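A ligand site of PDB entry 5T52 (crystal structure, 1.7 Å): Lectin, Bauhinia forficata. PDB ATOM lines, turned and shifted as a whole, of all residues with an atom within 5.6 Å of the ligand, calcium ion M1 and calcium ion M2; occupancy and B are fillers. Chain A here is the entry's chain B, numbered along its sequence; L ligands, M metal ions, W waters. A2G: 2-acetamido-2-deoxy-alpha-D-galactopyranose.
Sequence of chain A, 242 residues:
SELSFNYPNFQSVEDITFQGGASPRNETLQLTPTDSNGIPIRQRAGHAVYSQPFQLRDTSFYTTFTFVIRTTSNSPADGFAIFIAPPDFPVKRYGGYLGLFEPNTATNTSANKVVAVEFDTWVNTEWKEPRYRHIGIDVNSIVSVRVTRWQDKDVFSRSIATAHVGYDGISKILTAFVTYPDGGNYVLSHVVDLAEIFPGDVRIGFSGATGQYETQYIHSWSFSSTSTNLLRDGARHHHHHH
The backbone NH (N) of Gly 95 is in hydrogen-bond range of the backbone carbonyl oxygen (O) of Thr 210 (2.9 Å).
NE1 of Trp 127 sits close to OE1 of Glu 129, at 3.1 Å.
N of Ala 77 sits at hydrogen-bond distance from O of Gln 212, at 2.9 Å.
ND2 of Asn 124 sits at hydrogen-bond distance from OE1 of Glu 126, at 2.9 Å.
The backbone NH (N) of Gly 96 lies within hydrogen-bond range of the side-chain carboxylate (OD1) of Asp 78, 3.3 Å away.
O of Asp 78 sits at hydrogen-bond distance from N of Thr 121 (3.1 Å).
The side-chain carboxylate (OD2) of Asp 78 sits close to the backbone NH (N) of Gly 211.
Of the 23 residues printed, 4 come within 4 Å of calcium ion M2.
The nearest printed residue that does not touch calcium ion M2 is Ser 144 (4.3 Å).
Residues that only touch the ligand: Ala 77, Gly 95, Tyr 97, Trp 127 and Gly 211.
Hydrophobic or aromatic side chains that line the ligand: Ala 77, Tyr 97, Trp 122 and Trp 127.
11 residues have an atom within 4 Å of the ligand: Ala 77, Asp 78, Gly 95, Gly 96, Tyr 97, Trp 122, Asn 124, Glu 126, Trp 127, Gly 211 and Gln 212.
Four residues have an atom within 4 Å of calcium ion M1: Asp 120, Trp 122, Asn 124 and Glu 129.
The side-chain carboxylate (OD2) of Asp 120 binds calcium ion M2 (2.3 Å).
The side-chain carboxylate (OE2) of Glu 118 is bound to calcium ion M2.
Water W9 is bound to calcium ion M2.
Calcium ion M2 is bound by OE1 of Glu 129.
Water W6 binds calcium ion M2.
Calcium ion M2 is bound by NE2 of His 134 (2.4 Å).
An oxygen (O4) of the ligand is in hydrogen-bond range of the side-chain carboxylate of Asp 78 (2.5 Å).
The side-chain amide oxygen of Gln 212 lies within hydrogen-bond range of an oxygen (O6) of the ligand.
OE2 of Glu 126 sits at hydrogen-bond distance from N2 of the ligand (3.1 Å).
ND2 of Asn 124 lies within hydrogen-bond range of O3 of the ligand (2.9 Å).
The backbone NH of Gly 96 lies within hydrogen-bond range of an oxygen (O3) of the ligand (2.8 Å).
Calcium ion M1 is bound by O of Trp 122, water W7, OD1 of Asn 124, water W3, OE2 of Glu 129, OD2 of Asp 120 and OD1 of Asp 120.
Calcium ion M1 has seven donor atoms within binding distance.
Water W6 lies within hydrogen-bond range of the side-chain carboxylate of Glu 118 (2.7 Å) and the backbone carbonyl oxygen of Ile 142 (2.8 Å).
Water W2 bridges an oxygen (O7) of the ligand and the backbone carbonyl oxygen (O) of Tyr 94.
Water W1 bridges an oxygen (O4) of the ligand and the backbone NH (N) of Gly 211.
Water W8 lies within hydrogen-bond range of the side-chain carboxylate (OE2) of Glu 126 (2.9 Å), the indole nitrogen (NE1) of Trp 122 (3.0 Å) and an oxygen (O1) of the ligand (3.3 Å).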
ATOM      1  N   ALA A  77      20.687 -10.337  16.854  1.00  0.00           N
ATOM      2  CA  ALA A  77      20.588  -8.920  17.190  1.00  0.00           C
ATOM      3  C   ALA A  77      21.885  -8.257  16.749  1.00  0.00           C
ATOM      4  O   ALA A  77      22.923  -8.885  16.861  1.00  0.00           O
ATOM      5  CB  ALA A  77      20.391  -8.738  18.689  1.00  0.00           C
ATOM      6  N   ASP A  78      21.928  -6.998  16.353  1.00  0.00           N
ATOM      7  CA  ASP A  78      20.780  -6.040  16.435  1.00  0.00           C
ATOM      8  C   ASP A  78      20.382  -5.448  15.109  1.00  0.00           C
ATOM      9  O   ASP A  78      19.297  -4.833  15.021  1.00  0.00           O
ATOM     10  CB  ASP A  78      21.146  -4.895  17.331  1.00  0.00           C
ATOM     11  CG  ASP A  78      20.879  -5.223  18.778  1.00  0.00           C
ATOM     12  OD1 ASP A  78      19.721  -4.945  19.173  1.00  0.00           O
ATOM     13  OD2 ASP A  78      21.769  -5.732  19.533  1.00  0.00           O
ATOM     14  N   TYR A  94      26.769  -0.095  21.087  1.00  0.00           N
ATOM     15  CA  TYR A  94      26.365  -1.387  20.590  1.00  0.00           C
ATOM     16  C   TYR A  94      24.989  -1.770  21.025  1.00  0.00           C
ATOM     17  O   TYR A  94      24.253  -0.956  21.591  1.00  0.00           O
ATOM     18  CB  TYR A  94      27.463  -2.433  20.980  1.00  0.00           C
ATOM     19  CG  TYR A  94      27.746  -2.405  22.483  1.00  0.00           C
ATOM     20  CD1 TYR A  94      26.807  -2.827  23.411  1.00  0.00           C
ATOM     21  CD2 TYR A  94      28.857  -1.767  22.981  1.00  0.00           C
ATOM     22  CE1 TYR A  94      27.018  -2.760  24.813  1.00  0.00           C
ATOM     23  CE2 TYR A  94      29.056  -1.664  24.350  1.00  0.00           C
ATOM     24  CZ  TYR A  94      28.162  -2.141  25.261  1.00  0.00           C
ATOM     25  OH  TYR A  94      28.369  -2.009  26.620  1.00  0.00           O
ATOM     26  N   GLY A  95      24.544  -2.964  20.701  1.00  0.00           N
ATOM     27  CA  GLY A  95      23.203  -3.413  21.041  1.00  0.00           C
ATOM     28  C   GLY A  95      22.154  -2.679  20.172  1.00  0.00           C
ATOM     29  O   GLY A  95      22.410  -2.342  19.029  1.00  0.00           O
ATOM     30  N   GLY A  96      21.004  -2.396  20.729  1.00  0.00           N
ATOM     31  CA  GLY A  96      19.887  -1.813  20.031  1.00  0.00           C
ATOM     32  C   GLY A  96      20.087  -0.364  19.584  1.00  0.00           C
ATOM     33  O   GLY A  96      19.351   0.178  18.710  1.00  0.00           O
ATOM     34  N   TYR A  97      21.122   0.248  20.122  1.00  0.00           N
ATOM     35  CA  TYR A  97      21.489   1.609  19.661  1.00  0.00           C
ATOM     36  C   TYR A  97      22.096   1.621  18.227  1.00  0.00           C
ATOM     37  O   TYR A  97      22.388   2.701  17.690  1.00  0.00           O
ATOM     38  CB  TYR A  97      22.382   2.262  20.660  1.00  0.00           C
ATOM     39  CG  TYR A  97      21.754   2.370  22.022  1.00  0.00           C
ATOM     40  CD1 TYR A  97      20.708   3.261  22.276  1.00  0.00           C
ATOM     41  CD2 TYR A  97      22.092   1.450  23.033  1.00  0.00           C
ATOM     42  CE1 TYR A  97      20.106   3.318  23.531  1.00  0.00           C
ATOM     43  CE2 TYR A  97      21.495   1.504  24.233  1.00  0.00           C
ATOM     44  CZ  TYR A  97      20.458   2.404  24.440  1.00  0.00           C
ATOM     45  OH  TYR A  97      19.818   2.465  25.656  1.00  0.00           O
ATOM     46  N   LEU A  98      22.419   0.415  17.684  1.00  0.00           N
ATOM     47  CA  LEU A  98      22.939   0.196  16.321  1.00  0.00           C
ATOM     48  C   LEU A  98      24.225   0.940  15.945  1.00  0.00           C
ATOM     49  O   LEU A  98      24.527   1.102  14.805  1.00  0.00           O
ATOM     50  CB  LEU A  98      21.795   0.524  15.298  1.00  0.00           C
ATOM     51  CG  LEU A  98      20.595  -0.470  15.378  1.00  0.00           C
ATOM     52  CD1 LEU A  98      19.452   0.093  14.494  1.00  0.00           C
ATOM     53  CD2 LEU A  98      20.987  -1.823  14.868  1.00  0.00           C
ATOM     54  N   GLU A 118      17.529   1.979   8.750  1.00  0.00           N
ATOM     55  CA  GLU A 118      17.961   0.948   9.638  1.00  0.00           C
ATOM     56  C   GLU A 118      17.254  -0.353   9.252  1.00  0.00           C
ATOM     57  O   GLU A 118      16.140  -0.330   8.782  1.00  0.00           O
ATOM     58  CB  GLU A 118      17.652   1.245  11.102  1.00  0.00           C
ATOM     59  CG  GLU A 118      16.187   1.589  11.491  1.00  0.00           C
ATOM     60  CD  GLU A 118      15.953   1.441  12.975  1.00  0.00           C
ATOM     61  OE1 GLU A 118      16.625   2.218  13.640  1.00  0.00           O
ATOM     62  OE2 GLU A 118      15.103   0.607  13.356  1.00  0.00           O
ATOM     63  N   ASP A 120      16.480  -3.582  11.299  1.00  0.00           N
ATOM     64  CA  ASP A 120      16.462  -3.870  12.728  1.00  0.00           C
ATOM     65  C   ASP A 120      15.985  -5.292  12.957  1.00  0.00           C
ATOM     66  O   ASP A 120      14.824  -5.631  12.758  1.00  0.00           O
ATOM     67  CB  ASP A 120      15.535  -2.857  13.423  1.00  0.00           C
ATOM     68  CG  ASP A 120      15.662  -2.866  14.897  1.00  0.00           C
ATOM     69  OD1 ASP A 120      16.012  -3.955  15.364  1.00  0.00           O
ATOM     70  OD2 ASP A 120      15.424  -1.796  15.521  1.00  0.00           O
ATOM     71  N   THR A 121      16.924  -6.134  13.427  1.00  0.00           N
ATOM     72  CA  THR A 121      16.633  -7.550  13.629  1.00  0.00           C
ATOM     73  C   THR A 121      16.134  -7.919  15.020  1.00  0.00           C
ATOM     74  O   THR A 121      15.813  -9.121  15.288  1.00  0.00           O
ATOM     75  CB  THR A 121      17.897  -8.384  13.337  1.00  0.00           C
ATOM     76  OG1 THR A 121      18.955  -8.025  14.252  1.00  0.00           O
ATOM     77  CG2 THR A 121      18.269  -8.254  11.971  1.00  0.00           C
ATOM     78  N   TRP A 122      16.139  -6.947  15.940  1.00  0.00           N
ATOM     79  CA  TRP A 122      15.815  -7.175  17.333  1.00  0.00           C
ATOM     80  C   TRP A 122      14.841  -6.169  17.909  1.00  0.00           C
ATOM     81  O   TRP A 122      15.056  -4.964  18.029  1.00  0.00           O
ATOM     82  CB  TRP A 122      17.084  -7.246  18.182  1.00  0.00           C
ATOM     83  CG  TRP A 122      16.858  -7.431  19.685  1.00  0.00           C
ATOM     84  CD1 TRP A 122      16.531  -6.481  20.561  1.00  0.00           C
ATOM     85  CD2 TRP A 122      16.858  -8.680  20.440  1.00  0.00           C
ATOM     86  NE1 TRP A 122      16.342  -7.029  21.835  1.00  0.00           N
ATOM     87  CE2 TRP A 122      16.567  -8.364  21.764  1.00  0.00           C
ATOM     88  CE3 TRP A 122      17.151  -9.993  20.107  1.00  0.00           C
ATOM     89  CZ2 TRP A 122      16.504  -9.346  22.793  1.00  0.00           C
ATOM     90  CZ3 TRP A 122      17.081 -10.987  21.115  1.00  0.00           C
ATOM     91  CH2 TRP A 122      16.826 -10.630  22.458  1.00  0.00           C
ATOM     92  N   VAL A 123      13.739  -6.748  18.314  1.00  0.00           N
ATOM     93  CA  VAL A 123      12.662  -5.931  18.937  1.00  0.00           C
ATOM     94  C   VAL A 123      13.058  -5.503  20.327  1.00  0.00           C
ATOM     95  O   VAL A 123      13.089  -6.322  21.214  1.00  0.00           O
ATOM     96  CB  VAL A 123      11.336  -6.712  18.945  1.00  0.00           C
ATOM     97  CG1 VAL A 123      10.253  -5.939  19.689  1.00  0.00           C
ATOM     98  CG2 VAL A 123      10.924  -6.939  17.482  1.00  0.00           C
ATOM     99  N   ASN A 124      13.300  -4.189  20.477  1.00  0.00           N
ATOM    100  CA  ASN A 124      13.624  -3.583  21.737  1.00  0.00           C
ATOM    101  C   ASN A 124      12.375  -3.064  22.429  1.00  0.00           C
ATOM    102  O   ASN A 124      11.535  -2.442  21.793  1.00  0.00           O
ATOM    103  CB  ASN A 124      14.598  -2.413  21.506  1.00  0.00           C
ATOM    104  CG  ASN A 124      15.935  -2.884  21.091  1.00  0.00           C
ATOM    105  OD1 ASN A 124      16.345  -2.905  19.933  1.00  0.00           O
ATOM    106  ND2 ASN A 124      16.726  -3.230  22.152  1.00  0.00           N
ATOM    107  N   GLU A 126      13.016  -1.255  25.247  1.00  0.00           N
ATOM    108  CA  GLU A 126      13.563  -0.100  25.939  1.00  0.00           C
ATOM    109  C   GLU A 126      13.126   1.263  25.411  1.00  0.00           C
ATOM    110  O   GLU A 126      13.332   2.259  26.083  1.00  0.00           O
ATOM    111  CB  GLU A 126      15.074  -0.179  25.980  1.00  0.00           C
ATOM    112  CG  GLU A 126      15.635  -1.413  26.648  1.00  0.00           C
ATOM    113  CD  GLU A 126      15.929  -2.582  25.719  1.00  0.00           C
ATOM    114  OE1 GLU A 126      15.291  -2.656  24.636  1.00  0.00           O
ATOM    115  OE2 GLU A 126      16.730  -3.497  26.101  1.00  0.00           O
ATOM    116  N   TRP A 127      12.566   1.303  24.190  1.00  0.00           N
ATOM    117  CA  TRP A 127      12.061   2.520  23.562  1.00  0.00           C
ATOM    118  C   TRP A 127      10.977   2.002  22.617  1.00  0.00           C
ATOM    119  O   TRP A 127      10.863   0.801  22.418  1.00  0.00           O
ATOM    120  CB  TRP A 127      13.147   3.320  22.763  1.00  0.00           C
ATOM    121  CG  TRP A 127      13.952   2.502  21.867  1.00  0.00           C
ATOM    122  CD1 TRP A 127      13.595   2.056  20.568  1.00  0.00           C
ATOM    123  CD2 TRP A 127      15.177   1.887  22.168  1.00  0.00           C
ATOM    124  NE1 TRP A 127      14.601   1.289  20.082  1.00  0.00           N
ATOM    125  CE2 TRP A 127      15.578   1.152  21.038  1.00  0.00           C
ATOM    126  CE3 TRP A 127      16.028   1.929  23.298  1.00  0.00           C
ATOM    127  CZ2 TRP A 127      16.799   0.463  20.966  1.00  0.00           C
ATOM    128  CZ3 TRP A 127      17.240   1.256  23.274  1.00  0.00           C
ATOM    129  CH2 TRP A 127      17.612   0.505  22.094  1.00  0.00           C
ATOM    130  N   GLU A 129       9.221   0.810  19.445  1.00  0.00           N
ATOM    131  CA  GLU A 129       9.369   0.310  18.069  1.00  0.00           C
ATOM    132  C   GLU A 129       8.450  -0.871  17.840  1.00  0.00           C
ATOM    133  O   GLU A 129       7.895  -1.407  18.776  1.00  0.00           O
ATOM    134  CB  GLU A 129      10.860  -0.015  17.739  1.00  0.00           C
ATOM    135  CG  GLU A 129      11.637  -1.078  18.560  1.00  0.00           C
ATOM    136  CD  GLU A 129      13.040  -1.294  18.068  1.00  0.00           C
ATOM    137  OE1 GLU A 129      13.731  -0.331  17.638  1.00  0.00           O
ATOM    138  OE2 GLU A 129      13.550  -2.395  18.217  1.00  0.00           O
ATOM    139  N   PRO A 130       8.241  -1.246  16.589  1.00  0.00           N
ATOM    140  CA  PRO A 130       7.325  -2.371  16.405  1.00  0.00           C
ATOM    141  C   PRO A 130       7.669  -3.647  17.057  1.00  0.00           C
ATOM    142  O   PRO A 130       8.834  -3.932  17.363  1.00  0.00           O
ATOM    143  CB  PRO A 130       7.313  -2.567  14.881  1.00  0.00           C
ATOM    144  CG  PRO A 130       7.914  -1.328  14.330  1.00  0.00           C
ATOM    145  CD  PRO A 130       8.804  -0.769  15.336  1.00  0.00           C
ATOM    146  N   HIS A 134      11.917  -5.001  11.501  1.00  0.00           N
ATOM    147  CA  HIS A 134      11.442  -3.826  10.765  1.00  0.00           C
ATOM    148  C   HIS A 134      12.591  -3.102  10.093  1.00  0.00           C
ATOM    149  O   HIS A 134      13.761  -3.212  10.437  1.00  0.00           O
ATOM    150  CB  HIS A 134      10.653  -2.806  11.577  1.00  0.00           C
ATOM    151  CG  HIS A 134      11.323  -2.422  12.857  1.00  0.00           C
ATOM    152  ND1 HIS A 134      11.365  -3.225  13.972  1.00  0.00           N
ATOM    153  CD2 HIS A 134      12.111  -1.350  13.144  1.00  0.00           C
ATOM    154  CE1 HIS A 134      12.071  -2.642  14.922  1.00  0.00           C
ATOM    155  NE2 HIS A 134      12.532  -1.500  14.455  1.00  0.00           N
ATOM    156  N   ILE A 142      16.581   7.074  17.801  1.00  0.00           N
ATOM    157  CA  ILE A 142      16.442   5.680  17.645  1.00  0.00           C
ATOM    158  C   ILE A 142      14.993   5.224  17.438  1.00  0.00           C
ATOM    159  O   ILE A 142      14.803   4.069  17.109  1.00  0.00           O
ATOM    160  CB  ILE A 142      17.109   4.894  18.822  1.00  0.00           C
ATOM    161  CG1 ILE A 142      17.417   3.429  18.504  1.00  0.00           C
ATOM    162  CG2 ILE A 142      16.249   5.046  20.077  1.00  0.00           C
ATOM    163  CD1 ILE A 142      18.248   3.117  17.264  1.00  0.00           C
ATOM    164  N   SER A 144      12.190   5.322  15.104  1.00  0.00           N
ATOM    165  CA  SER A 144      12.066   5.682  13.695  1.00  0.00           C
ATOM    166  C   SER A 144      10.899   6.578  13.416  1.00  0.00           C
ATOM    167  O   SER A 144       9.841   6.343  13.984  1.00  0.00           O
ATOM    168  CB  SER A 144      11.907   4.400  12.845  1.00  0.00           C
ATOM    169  OG  SER A 144      13.060   3.522  12.994  1.00  0.00           O
ATOM    170  N   THR A 210      26.024  -5.635  17.402  1.00  0.00           N
ATOM    171  CA  THR A 210      25.522  -6.787  18.159  1.00  0.00           C
ATOM    172  C   THR A 210      25.423  -6.346  19.637  1.00  0.00           C
ATOM    173  O   THR A 210      25.993  -5.340  20.034  1.00  0.00           O
ATOM    174  CB  THR A 210      26.545  -7.972  18.109  1.00  0.00           C
ATOM    175  OG1 THR A 210      27.799  -7.460  18.622  1.00  0.00           O
ATOM    176  CG2 THR A 210      26.786  -8.446  16.687  1.00  0.00           C
ATOM    177  N   GLY A 211      24.663  -7.053  20.446  1.00  0.00           N
ATOM    178  CA  GLY A 211      23.759  -8.166  20.123  1.00  0.00           C
ATOM    179  C   GLY A 211      24.411  -9.524  20.174  1.00  0.00           C
ATOM    180  O   GLY A 211      25.172  -9.794  21.097  1.00  0.00           O
ATOM    181  N   GLN A 212      24.079 -10.361  19.234  1.00  0.00           N
ATOM    182  CA  GLN A 212      24.253 -11.824  19.328  1.00  0.00           C
ATOM    183  C   GLN A 212      23.884 -12.551  18.036  1.00  0.00           C
ATOM    184  O   GLN A 212      22.894 -12.167  17.358  1.00  0.00           O
ATOM    185  CB  GLN A 212      23.396 -12.403  20.449  1.00  0.00           C
ATOM    186  CG  GLN A 212      21.929 -12.060  20.480  1.00  0.00           C
ATOM    187  CD  GLN A 212      21.141 -12.655  21.622  1.00  0.00           C
ATOM    188  OE1 GLN A 212      21.551 -12.577  22.769  1.00  0.00           O
ATOM    189  NE2 GLN A 212      20.026 -13.252  21.313  1.00  0.00           N
HETATM  190  O5  A2G L   1      20.689  -7.472  24.433  1.00  0.00           O
HETATM  191  C1  A2G L   1      20.214  -6.219  25.015  1.00  0.00           C
HETATM  192  O1  A2G L   1      18.967  -6.405  25.641  1.00  0.00           O
HETATM  193  C2  A2G L   1      20.036  -5.109  23.966  1.00  0.00           C
HETATM  194  N2  A2G L   1      19.445  -3.943  24.579  1.00  0.00           N
HETATM  195  C3  A2G L   1      19.265  -5.584  22.690  1.00  0.00           C
HETATM  196  O3  A2G L   1      19.344  -4.472  21.748  1.00  0.00           O
HETATM  197  C4  A2G L   1      19.918  -6.885  22.196  1.00  0.00           C
HETATM  198  O4  A2G L   1      21.252  -6.675  21.787  1.00  0.00           O
HETATM  199  C5  A2G L   1      19.869  -7.898  23.301  1.00  0.00           C
HETATM  200  C6  A2G L   1      20.329  -9.289  22.880  1.00  0.00           C
HETATM  201  O6  A2G L   1      20.377 -10.146  24.044  1.00  0.00           O
HETATM  202  C7  A2G L   1      19.914  -2.718  24.425  1.00  0.00           C
HETATM  203  O7  A2G L   1      20.938  -2.494  23.756  1.00  0.00           O
HETATM  204  C8  A2G L   1      19.176  -1.596  25.071  1.00  0.00           C
HETATM  205 CA    CA M   1      15.916  -2.903  17.703  1.00  0.00          CA
HETATM  206 CA    CA M   2      14.170   0.069  15.379  1.00  0.00          CA
HETATM  207  O   HOH W   1      23.616  -6.434  23.088  1.00  0.00           O
HETATM  208  O   HOH W   2      23.419  -1.613  24.236  1.00  0.00           O
HETATM  209  O   HOH W   3      18.075  -3.770  17.493  1.00  0.00           O
HETATM  210  O   HOH W   4      16.550  -8.061  26.306  1.00  0.00           O
HETATM  211  O   HOH W   5      18.373 -10.158  25.943  1.00  0.00           O
HETATM  212  O   HOH W   6      15.824   1.588  16.169  1.00  0.00           O
HETATM  213  O   HOH W   7      16.856  -0.840  17.754  1.00  0.00           O
HETATM  214  O   HOH W   8      15.960  -5.836  24.537  1.00  0.00           O
HETATM  215  O   HOH W   9      12.506   1.581  14.930  1.00  0.00           O
